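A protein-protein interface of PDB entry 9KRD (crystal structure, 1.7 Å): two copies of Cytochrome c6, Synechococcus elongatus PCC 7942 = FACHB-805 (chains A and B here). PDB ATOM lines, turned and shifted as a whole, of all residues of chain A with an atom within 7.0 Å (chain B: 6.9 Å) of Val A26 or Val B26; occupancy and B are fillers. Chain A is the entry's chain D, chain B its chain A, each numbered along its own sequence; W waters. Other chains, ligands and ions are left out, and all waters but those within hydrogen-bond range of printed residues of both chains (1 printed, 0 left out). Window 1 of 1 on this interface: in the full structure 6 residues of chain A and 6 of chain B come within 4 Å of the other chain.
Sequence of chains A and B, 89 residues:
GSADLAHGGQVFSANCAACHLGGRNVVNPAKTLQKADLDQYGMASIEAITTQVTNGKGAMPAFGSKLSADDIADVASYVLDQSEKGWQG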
ATOM      1  N   ALA A  17     -13.973 -14.138  13.918  1.00  0.00           N
ATOM      2  CA  ALA A  17     -15.126 -13.420  13.378  1.00  0.00           C
ATOM      3  C   ALA A  17     -15.672 -14.088  12.117  1.00  0.00           C
ATOM      4  O   ALA A  17     -16.859 -13.923  11.793  1.00  0.00           O
ATOM      5  CB  ALA A  17     -14.745 -11.970  13.101  1.00  0.00           C
ATOM      6  N   ALA A  18     -14.831 -14.832  11.393  1.00  0.00           N
ATOM      7  CA  ALA A  18     -15.316 -15.556  10.223  1.00  0.00           C
ATOM      8  C   ALA A  18     -16.518 -16.425  10.562  1.00  0.00           C
ATOM      9  O   ALA A  18     -17.415 -16.593   9.730  1.00  0.00           O
ATOM     10  CB  ALA A  18     -14.194 -16.417   9.625  1.00  0.00           C
ATOM     11  N   CYS A  19     -16.579 -16.955  11.784  1.00  0.00           N
ATOM     12  CA  CYS A  19     -17.720 -17.749  12.209  1.00  0.00           C
ATOM     13  C   CYS A  19     -18.547 -17.099  13.302  1.00  0.00           C
ATOM     14  O   CYS A  19     -19.751 -17.371  13.387  1.00  0.00           O
ATOM     15  CB  CYS A  19     -17.260 -19.123  12.705  1.00  0.00           C
ATOM     16  SG  CYS A  19     -16.488 -20.093  11.416  1.00  0.00           S
ATOM     17  N   HIS A  20     -17.949 -16.227  14.119  1.00  0.00           N
ATOM     18  CA  HIS A  20     -18.607 -15.698  15.314  1.00  0.00           C
ATOM     19  C   HIS A  20     -18.816 -14.188  15.273  1.00  0.00           C
ATOM     20  O   HIS A  20     -18.931 -13.558  16.334  1.00  0.00           O
ATOM     21  CB  HIS A  20     -17.808 -16.061  16.572  1.00  0.00           C
ATOM     22  CG  HIS A  20     -17.765 -17.531  16.869  1.00  0.00           C
ATOM     23  ND1 HIS A  20     -18.895 -18.286  17.110  1.00  0.00           N
ATOM     24  CD2 HIS A  20     -16.713 -18.376  17.002  1.00  0.00           C
ATOM     25  CE1 HIS A  20     -18.539 -19.534  17.373  1.00  0.00           C
ATOM     26  NE2 HIS A  20     -17.222 -19.617  17.302  1.00  0.00           N
ATOM     27  N   LEU A  21     -18.859 -13.596  14.080  1.00  0.00           N
ATOM     28  CA  LEU A  21     -19.114 -12.167  13.931  1.00  0.00           C
ATOM     29  C   LEU A  21     -20.240 -11.697  14.848  1.00  0.00           C
ATOM     30  O   LEU A  21     -21.324 -12.288  14.878  1.00  0.00           O
ATOM     31  CB  LEU A  21     -19.464 -11.864  12.471  1.00  0.00           C
ATOM     32  CG  LEU A  21     -19.644 -10.378  12.188  1.00  0.00           C
ATOM     33  CD1 LEU A  21     -18.306  -9.653  12.254  1.00  0.00           C
ATOM     34  CD2 LEU A  21     -20.300 -10.195  10.837  1.00  0.00           C
ATOM     35  N   ARG A  24     -22.207 -14.319  17.110  1.00  0.00           N
ATOM     36  CA  ARG A  24     -23.118 -15.325  16.575  1.00  0.00           C
ATOM     37  C   ARG A  24     -22.344 -16.611  16.298  1.00  0.00           C
ATOM     38  O   ARG A  24     -21.224 -16.791  16.786  1.00  0.00           O
ATOM     39  CB  ARG A  24     -23.800 -14.798  15.310  1.00  0.00           C
ATOM     40  CG  ARG A  24     -24.388 -13.415  15.454  1.00  0.00           C
ATOM     41  CD  ARG A  24     -25.456 -13.413  16.491  1.00  0.00           C
ATOM     42  NE  ARG A  24     -26.640 -14.129  16.035  1.00  0.00           N
ATOM     43  CZ  ARG A  24     -27.813 -14.049  16.646  1.00  0.00           C
ATOM     44  NH1 ARG A  24     -27.976 -13.295  17.724  1.00  0.00           N
ATOM     45  NH2 ARG A  24     -28.842 -14.739  16.165  1.00  0.00           N
ATOM     46  N   ASN A  25     -22.925 -17.510  15.499  1.00  0.00           N
ATOM     47  CA  ASN A  25     -22.222 -18.724  15.075  1.00  0.00           C
ATOM     48  C   ASN A  25     -22.805 -19.143  13.726  1.00  0.00           C
ATOM     49  O   ASN A  25     -23.878 -19.757  13.673  1.00  0.00           O
ATOM     50  CB  ASN A  25     -22.354 -19.835  16.104  1.00  0.00           C
ATOM     51  CG  ASN A  25     -21.516 -21.071  15.744  1.00  0.00           C
ATOM     52  OD1 ASN A  25     -21.224 -21.320  14.578  1.00  0.00           O
ATOM     53  ND2 ASN A  25     -21.143 -21.846  16.757  1.00  0.00           N
ATOM     54  N   VAL A  26     -22.065 -18.853  12.649  1.00  0.00           N
ATOM     55  CA  VAL A  26     -22.577 -19.084  11.302  1.00  0.00           C
ATOM     56  C   VAL A  26     -22.761 -20.563  11.009  1.00  0.00           C
ATOM     57  O   VAL A  26     -23.569 -20.918  10.144  1.00  0.00           O
ATOM     58  CB  VAL A  26     -21.648 -18.414  10.264  1.00  0.00           C
ATOM     59  CG1 VAL A  26     -20.375 -19.217  10.062  1.00  0.00           C
ATOM     60  CG2 VAL A  26     -22.371 -18.197   8.934  1.00  0.00           C
ATOM     61  N   VAL A  27     -22.031 -21.440  11.697  1.00  0.00           N
ATOM     62  CA  VAL A  27     -22.138 -22.874  11.442  1.00  0.00           C
ATOM     63  C   VAL A  27     -23.265 -23.501  12.246  1.00  0.00           C
ATOM     64  O   VAL A  27     -23.977 -24.372  11.746  1.00  0.00           O
ATOM     65  CB  VAL A  27     -20.797 -23.562  11.754  1.00  0.00           C
ATOM     66  CG1 VAL A  27     -20.879 -25.079  11.455  1.00  0.00           C
ATOM     67  CG2 VAL A  27     -19.683 -22.910  10.962  1.00  0.00           C
ATOM     68  N   ASN A  28     -23.420 -23.116  13.507  1.00  0.00           N
ATOM     69  CA  ASN A  28     -24.469 -23.670  14.363  1.00  0.00           C
ATOM     70  C   ASN A  28     -25.078 -22.572  15.219  1.00  0.00           C
ATOM     71  O   ASN A  28     -24.540 -22.237  16.284  1.00  0.00           O
ATOM     72  CB  ASN A  28     -23.955 -24.792  15.254  1.00  0.00           C
ATOM     73  CG  ASN A  28     -25.076 -25.434  16.056  1.00  0.00           C
ATOM     74  OD1 ASN A  28     -26.252 -25.049  15.933  1.00  0.00           O
ATOM     75  ND2 ASN A  28     -24.730 -26.426  16.865  1.00  0.00           N
ATOM     76  N   PRO A  29     -26.247 -22.060  14.836  1.00  0.00           N
ATOM     77  CA  PRO A  29     -26.850 -20.953  15.597  1.00  0.00           C
ATOM     78  C   PRO A  29     -27.253 -21.332  17.008  1.00  0.00           C
ATOM     79  O   PRO A  29     -27.600 -20.438  17.783  1.00  0.00           O
ATOM     80  CB  PRO A  29     -28.085 -20.572  14.764  1.00  0.00           C
ATOM     81  CG  PRO A  29     -28.053 -21.451  13.549  1.00  0.00           C
ATOM     82  CD  PRO A  29     -27.154 -22.594  13.808  1.00  0.00           C
ATOM     83  N   ALA B  17     -20.567 -31.282   5.288  1.00  0.00           N
ATOM     84  CA  ALA B  17     -21.801 -30.591   4.950  1.00  0.00           C
ATOM     85  C   ALA B  17     -22.152 -29.499   5.951  1.00  0.00           C
ATOM     86  O   ALA B  17     -22.952 -28.617   5.630  1.00  0.00           O
ATOM     87  CB  ALA B  17     -22.940 -31.607   4.841  1.00  0.00           C
ATOM     88  N   ALA B  18     -21.548 -29.517   7.146  1.00  0.00           N
ATOM     89  CA  ALA B  18     -21.819 -28.444   8.097  1.00  0.00           C
ATOM     90  C   ALA B  18     -21.415 -27.088   7.541  1.00  0.00           C
ATOM     91  O   ALA B  18     -21.993 -26.064   7.922  1.00  0.00           O
ATOM     92  CB  ALA B  18     -21.087 -28.714   9.410  1.00  0.00           C
ATOM     93  N   CYS B  19     -20.425 -27.059   6.638  1.00  0.00           N
ATOM     94  CA  CYS B  19     -19.987 -25.823   6.018  1.00  0.00           C
ATOM     95  C   CYS B  19     -20.123 -25.808   4.506  1.00  0.00           C
ATOM     96  O   CYS B  19     -20.141 -24.715   3.921  1.00  0.00           O
ATOM     97  CB  CYS B  19     -18.515 -25.534   6.385  1.00  0.00           C
ATOM     98  SG  CYS B  19     -18.217 -25.514   8.153  1.00  0.00           S
ATOM     99  N   HIS B  20     -20.280 -26.967   3.863  1.00  0.00           N
ATOM    100  CA  HIS B  20     -20.212 -27.060   2.410  1.00  0.00           C
ATOM    101  C   HIS B  20     -21.441 -27.741   1.810  1.00  0.00           C
ATOM    102  O   HIS B  20     -21.354 -28.290   0.707  1.00  0.00           O
ATOM    103  CB  HIS B  20     -18.956 -27.831   1.957  1.00  0.00           C
ATOM    104  CG  HIS B  20     -17.642 -27.187   2.306  1.00  0.00           C
ATOM    105  ND1 HIS B  20     -17.242 -25.961   1.810  1.00  0.00           N
ATOM    106  CD2 HIS B  20     -16.592 -27.659   3.021  1.00  0.00           C
ATOM    107  CE1 HIS B  20     -16.012 -25.697   2.229  1.00  0.00           C
ATOM    108  NE2 HIS B  20     -15.595 -26.711   2.970  1.00  0.00           N
ATOM    109  N   LEU B  21     -22.590 -27.708   2.485  1.00  0.00           N
ATOM    110  CA  LEU B  21     -23.774 -28.369   1.944  1.00  0.00           C
ATOM    111  C   LEU B  21     -24.030 -27.930   0.506  1.00  0.00           C
ATOM    112  O   LEU B  21     -24.059 -26.735   0.208  1.00  0.00           O
ATOM    113  CB  LEU B  21     -24.994 -28.063   2.809  1.00  0.00           C
ATOM    114  CG  LEU B  21     -26.236 -28.849   2.384  1.00  0.00           C
ATOM    115  CD1 LEU B  21     -26.058 -30.325   2.727  1.00  0.00           C
ATOM    116  CD2 LEU B  21     -27.442 -28.274   3.084  1.00  0.00           C
ATOM    117  N   ARG B  24     -21.580 -25.369  -1.187  1.00  0.00           N
ATOM    118  CA  ARG B  24     -21.425 -24.037  -0.615  1.00  0.00           C
ATOM    119  C   ARG B  24     -20.093 -23.901   0.120  1.00  0.00           C
ATOM    120  O   ARG B  24     -19.342 -24.862   0.304  1.00  0.00           O
ATOM    121  CB  ARG B  24     -22.541 -23.756   0.387  1.00  0.00           C
ATOM    122  CG  ARG B  24     -23.948 -23.623  -0.215  1.00  0.00           C
ATOM    123  CD  ARG B  24     -24.961 -23.607   0.916  1.00  0.00           C
ATOM    124  NE  ARG B  24     -26.336 -23.354   0.486  1.00  0.00           N
ATOM    125  CZ  ARG B  24     -27.193 -24.312   0.163  1.00  0.00           C
ATOM    126  NH1 ARG B  24     -26.822 -25.585   0.125  1.00  0.00           N
ATOM    127  NH2 ARG B  24     -28.457 -23.988  -0.128  1.00  0.00           N
ATOM    128  N   ASN B  25     -19.829 -22.681   0.580  1.00  0.00           N
ATOM    129  CA  ASN B  25     -18.914 -22.476   1.701  1.00  0.00           C
ATOM    130  C   ASN B  25     -19.552 -21.375   2.538  1.00  0.00           C
ATOM    131  O   ASN B  25     -19.435 -20.197   2.191  1.00  0.00           O
ATOM    132  CB  ASN B  25     -17.506 -22.104   1.255  1.00  0.00           C
ATOM    133  CG  ASN B  25     -16.544 -22.029   2.436  1.00  0.00           C
ATOM    134  OD1 ASN B  25     -16.978 -21.840   3.572  1.00  0.00           O
ATOM    135  ND2 ASN B  25     -15.245 -22.208   2.183  1.00  0.00           N
ATOM    136  N   VAL B  26     -20.267 -21.767   3.601  1.00  0.00           N
ATOM    137  CA  VAL B  26     -21.000 -20.777   4.388  1.00  0.00           C
ATOM    138  C   VAL B  26     -20.054 -19.929   5.215  1.00  0.00           C
ATOM    139  O   VAL B  26     -20.433 -18.843   5.648  1.00  0.00           O
ATOM    140  CB  VAL B  26     -22.051 -21.421   5.317  1.00  0.00           C
ATOM    141  CG1 VAL B  26     -23.042 -22.266   4.497  1.00  0.00           C
ATOM    142  CG2 VAL B  26     -21.381 -22.263   6.409  1.00  0.00           C
ATOM    143  N   VAL B  27     -18.835 -20.393   5.450  1.00  0.00           N
ATOM    144  CA  VAL B  27     -17.890 -19.635   6.274  1.00  0.00           C
ATOM    145  C   VAL B  27     -17.131 -18.602   5.458  1.00  0.00           C
ATOM    146  O   VAL B  27     -17.052 -17.423   5.830  1.00  0.00           O
ATOM    147  CB  VAL B  27     -16.917 -20.606   6.975  1.00  0.00           C
ATOM    148  CG1 VAL B  27     -15.847 -19.816   7.702  1.00  0.00           C
ATOM    149  CG2 VAL B  27     -17.670 -21.526   7.934  1.00  0.00           C
ATOM    150  N   ASN B  28     -16.539 -19.024   4.344  1.00  0.00           N
ATOM    151  CA  ASN B  28     -15.826 -18.133   3.435  1.00  0.00           C
ATOM    152  C   ASN B  28     -16.501 -18.249   2.077  1.00  0.00           C
ATOM    153  O   ASN B  28     -16.158 -19.132   1.278  1.00  0.00           O
ATOM    154  CB  ASN B  28     -14.336 -18.488   3.359  1.00  0.00           C
ATOM    155  CG  ASN B  28     -13.551 -17.514   2.512  1.00  0.00           C
ATOM    156  OD1 ASN B  28     -14.125 -16.753   1.724  1.00  0.00           O
ATOM    157  ND2 ASN B  28     -12.234 -17.518   2.671  1.00  0.00           N
ATOM    158  N   PRO B  29     -17.474 -17.381   1.776  1.00  0.00           N
ATOM    159  CA  PRO B  29     -18.248 -17.544   0.538  1.00  0.00           C
ATOM    160  C   PRO B  29     -17.434 -17.423  -0.741  1.00  0.00           C
ATOM    161  O   PRO B  29     -17.957 -17.746  -1.810  1.00  0.00           O
ATOM    162  CB  PRO B  29     -19.291 -16.420   0.629  1.00  0.00           C
ATOM    163  CG  PRO B  29     -19.478 -16.219   2.103  1.00  0.00           C
ATOM    164  CD  PRO B  29     -18.090 -16.418   2.702  1.00  0.00           C
ATOM    165  N   THR B  32     -15.931 -21.657  -2.446  1.00  0.00           N
ATOM    166  CA  THR B  32     -16.897 -22.744  -2.477  1.00  0.00           C
ATOM    167  C   THR B  32     -16.290 -23.974  -3.133  1.00  0.00           C
ATOM    168  O   THR B  32     -15.130 -23.981  -3.555  1.00  0.00           O
ATOM    169  CB  THR B  32     -18.166 -22.345  -3.231  1.00  0.00           C
ATOM    170  OG1 THR B  32     -17.901 -22.332  -4.644  1.00  0.00           O
ATOM    171  CG2 THR B  32     -18.659 -20.953  -2.778  1.00  0.00           C
HETATM  172  O   HOH W   1     -24.052 -26.057   9.332  1.00  0.00           O
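Of the 12 printed residues of chain B, 3 touch a printed residue of chain A. Hydrophobic or aromatic side chains of chain B that line the printed part of chain A: Val B27. Along chain A the printed residues that touch a printed residue of chain B span positions 19 to 27. Among the printed residues, 4 pairs touch across the chains.
The backbone NH (N) of Val B26 lies within hydrogen-bond range of the backbone carbonyl oxygen (O) of Cys B19 (3.0 Å). N of Val B27 lies within hydrogen-bond range of OD1 of Asn B25. O of Cys A19 sits at hydrogen-bond distance from N of Val A26, 2.8 Å away. OD1 of Asn A25 lies within hydrogen-bond range of N of Val A27, 3.0 Å away.
Cys A19 touches Val B27, but with the chains exchanged Val A27 does not touch Cys B19 (4.1 Å). Val B26 touches its own counterpart, Val A26. Val A27 touches Ala B18, but with the chains exchanged Ala A18 does not touch Val B27 (4.004 Å). Val A27 touches its own counterpart, Val B27. Of the 4 pairs that touch across the chains among the printed residues, 2 have their exchanged pair printed and touching as well.
Water W1 lies within hydrogen-bond range of the backbone carbonyl oxygen of Ala B18 (2.5 Å) and the backbone carbonyl oxygen of Val A27 (2.9 Å).
Of the printed residues of chain B, Cys A19 touches Val B27 (3.8 Å). Of the printed residues of chain B, Val A26 touches Val B26 (3.9 Å). Of the printed residues of chain B, Val A27 touches Ala B18 (3.8 Å) and Val B27 (3.9 Å). Asn A28 touches none of the printed residues of chain B. Printed residues of chain A within 4 Å of Ala B18: Val A27. His B20 touches none of the printed residues of chain A. Of chain A, only Val A26 comes within 4 Å of Val B26. Printed residues of chain A within 4 Å of Val B27: Cys A19 and Val A27.
Cys A19 touches Val B27 (SG to CG1, 3.8 Å). Val B26 touches Val A26. CG1 of Val A27 touches O of Ala B18, 3.8 Å away. Val B27 touches Val A27.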
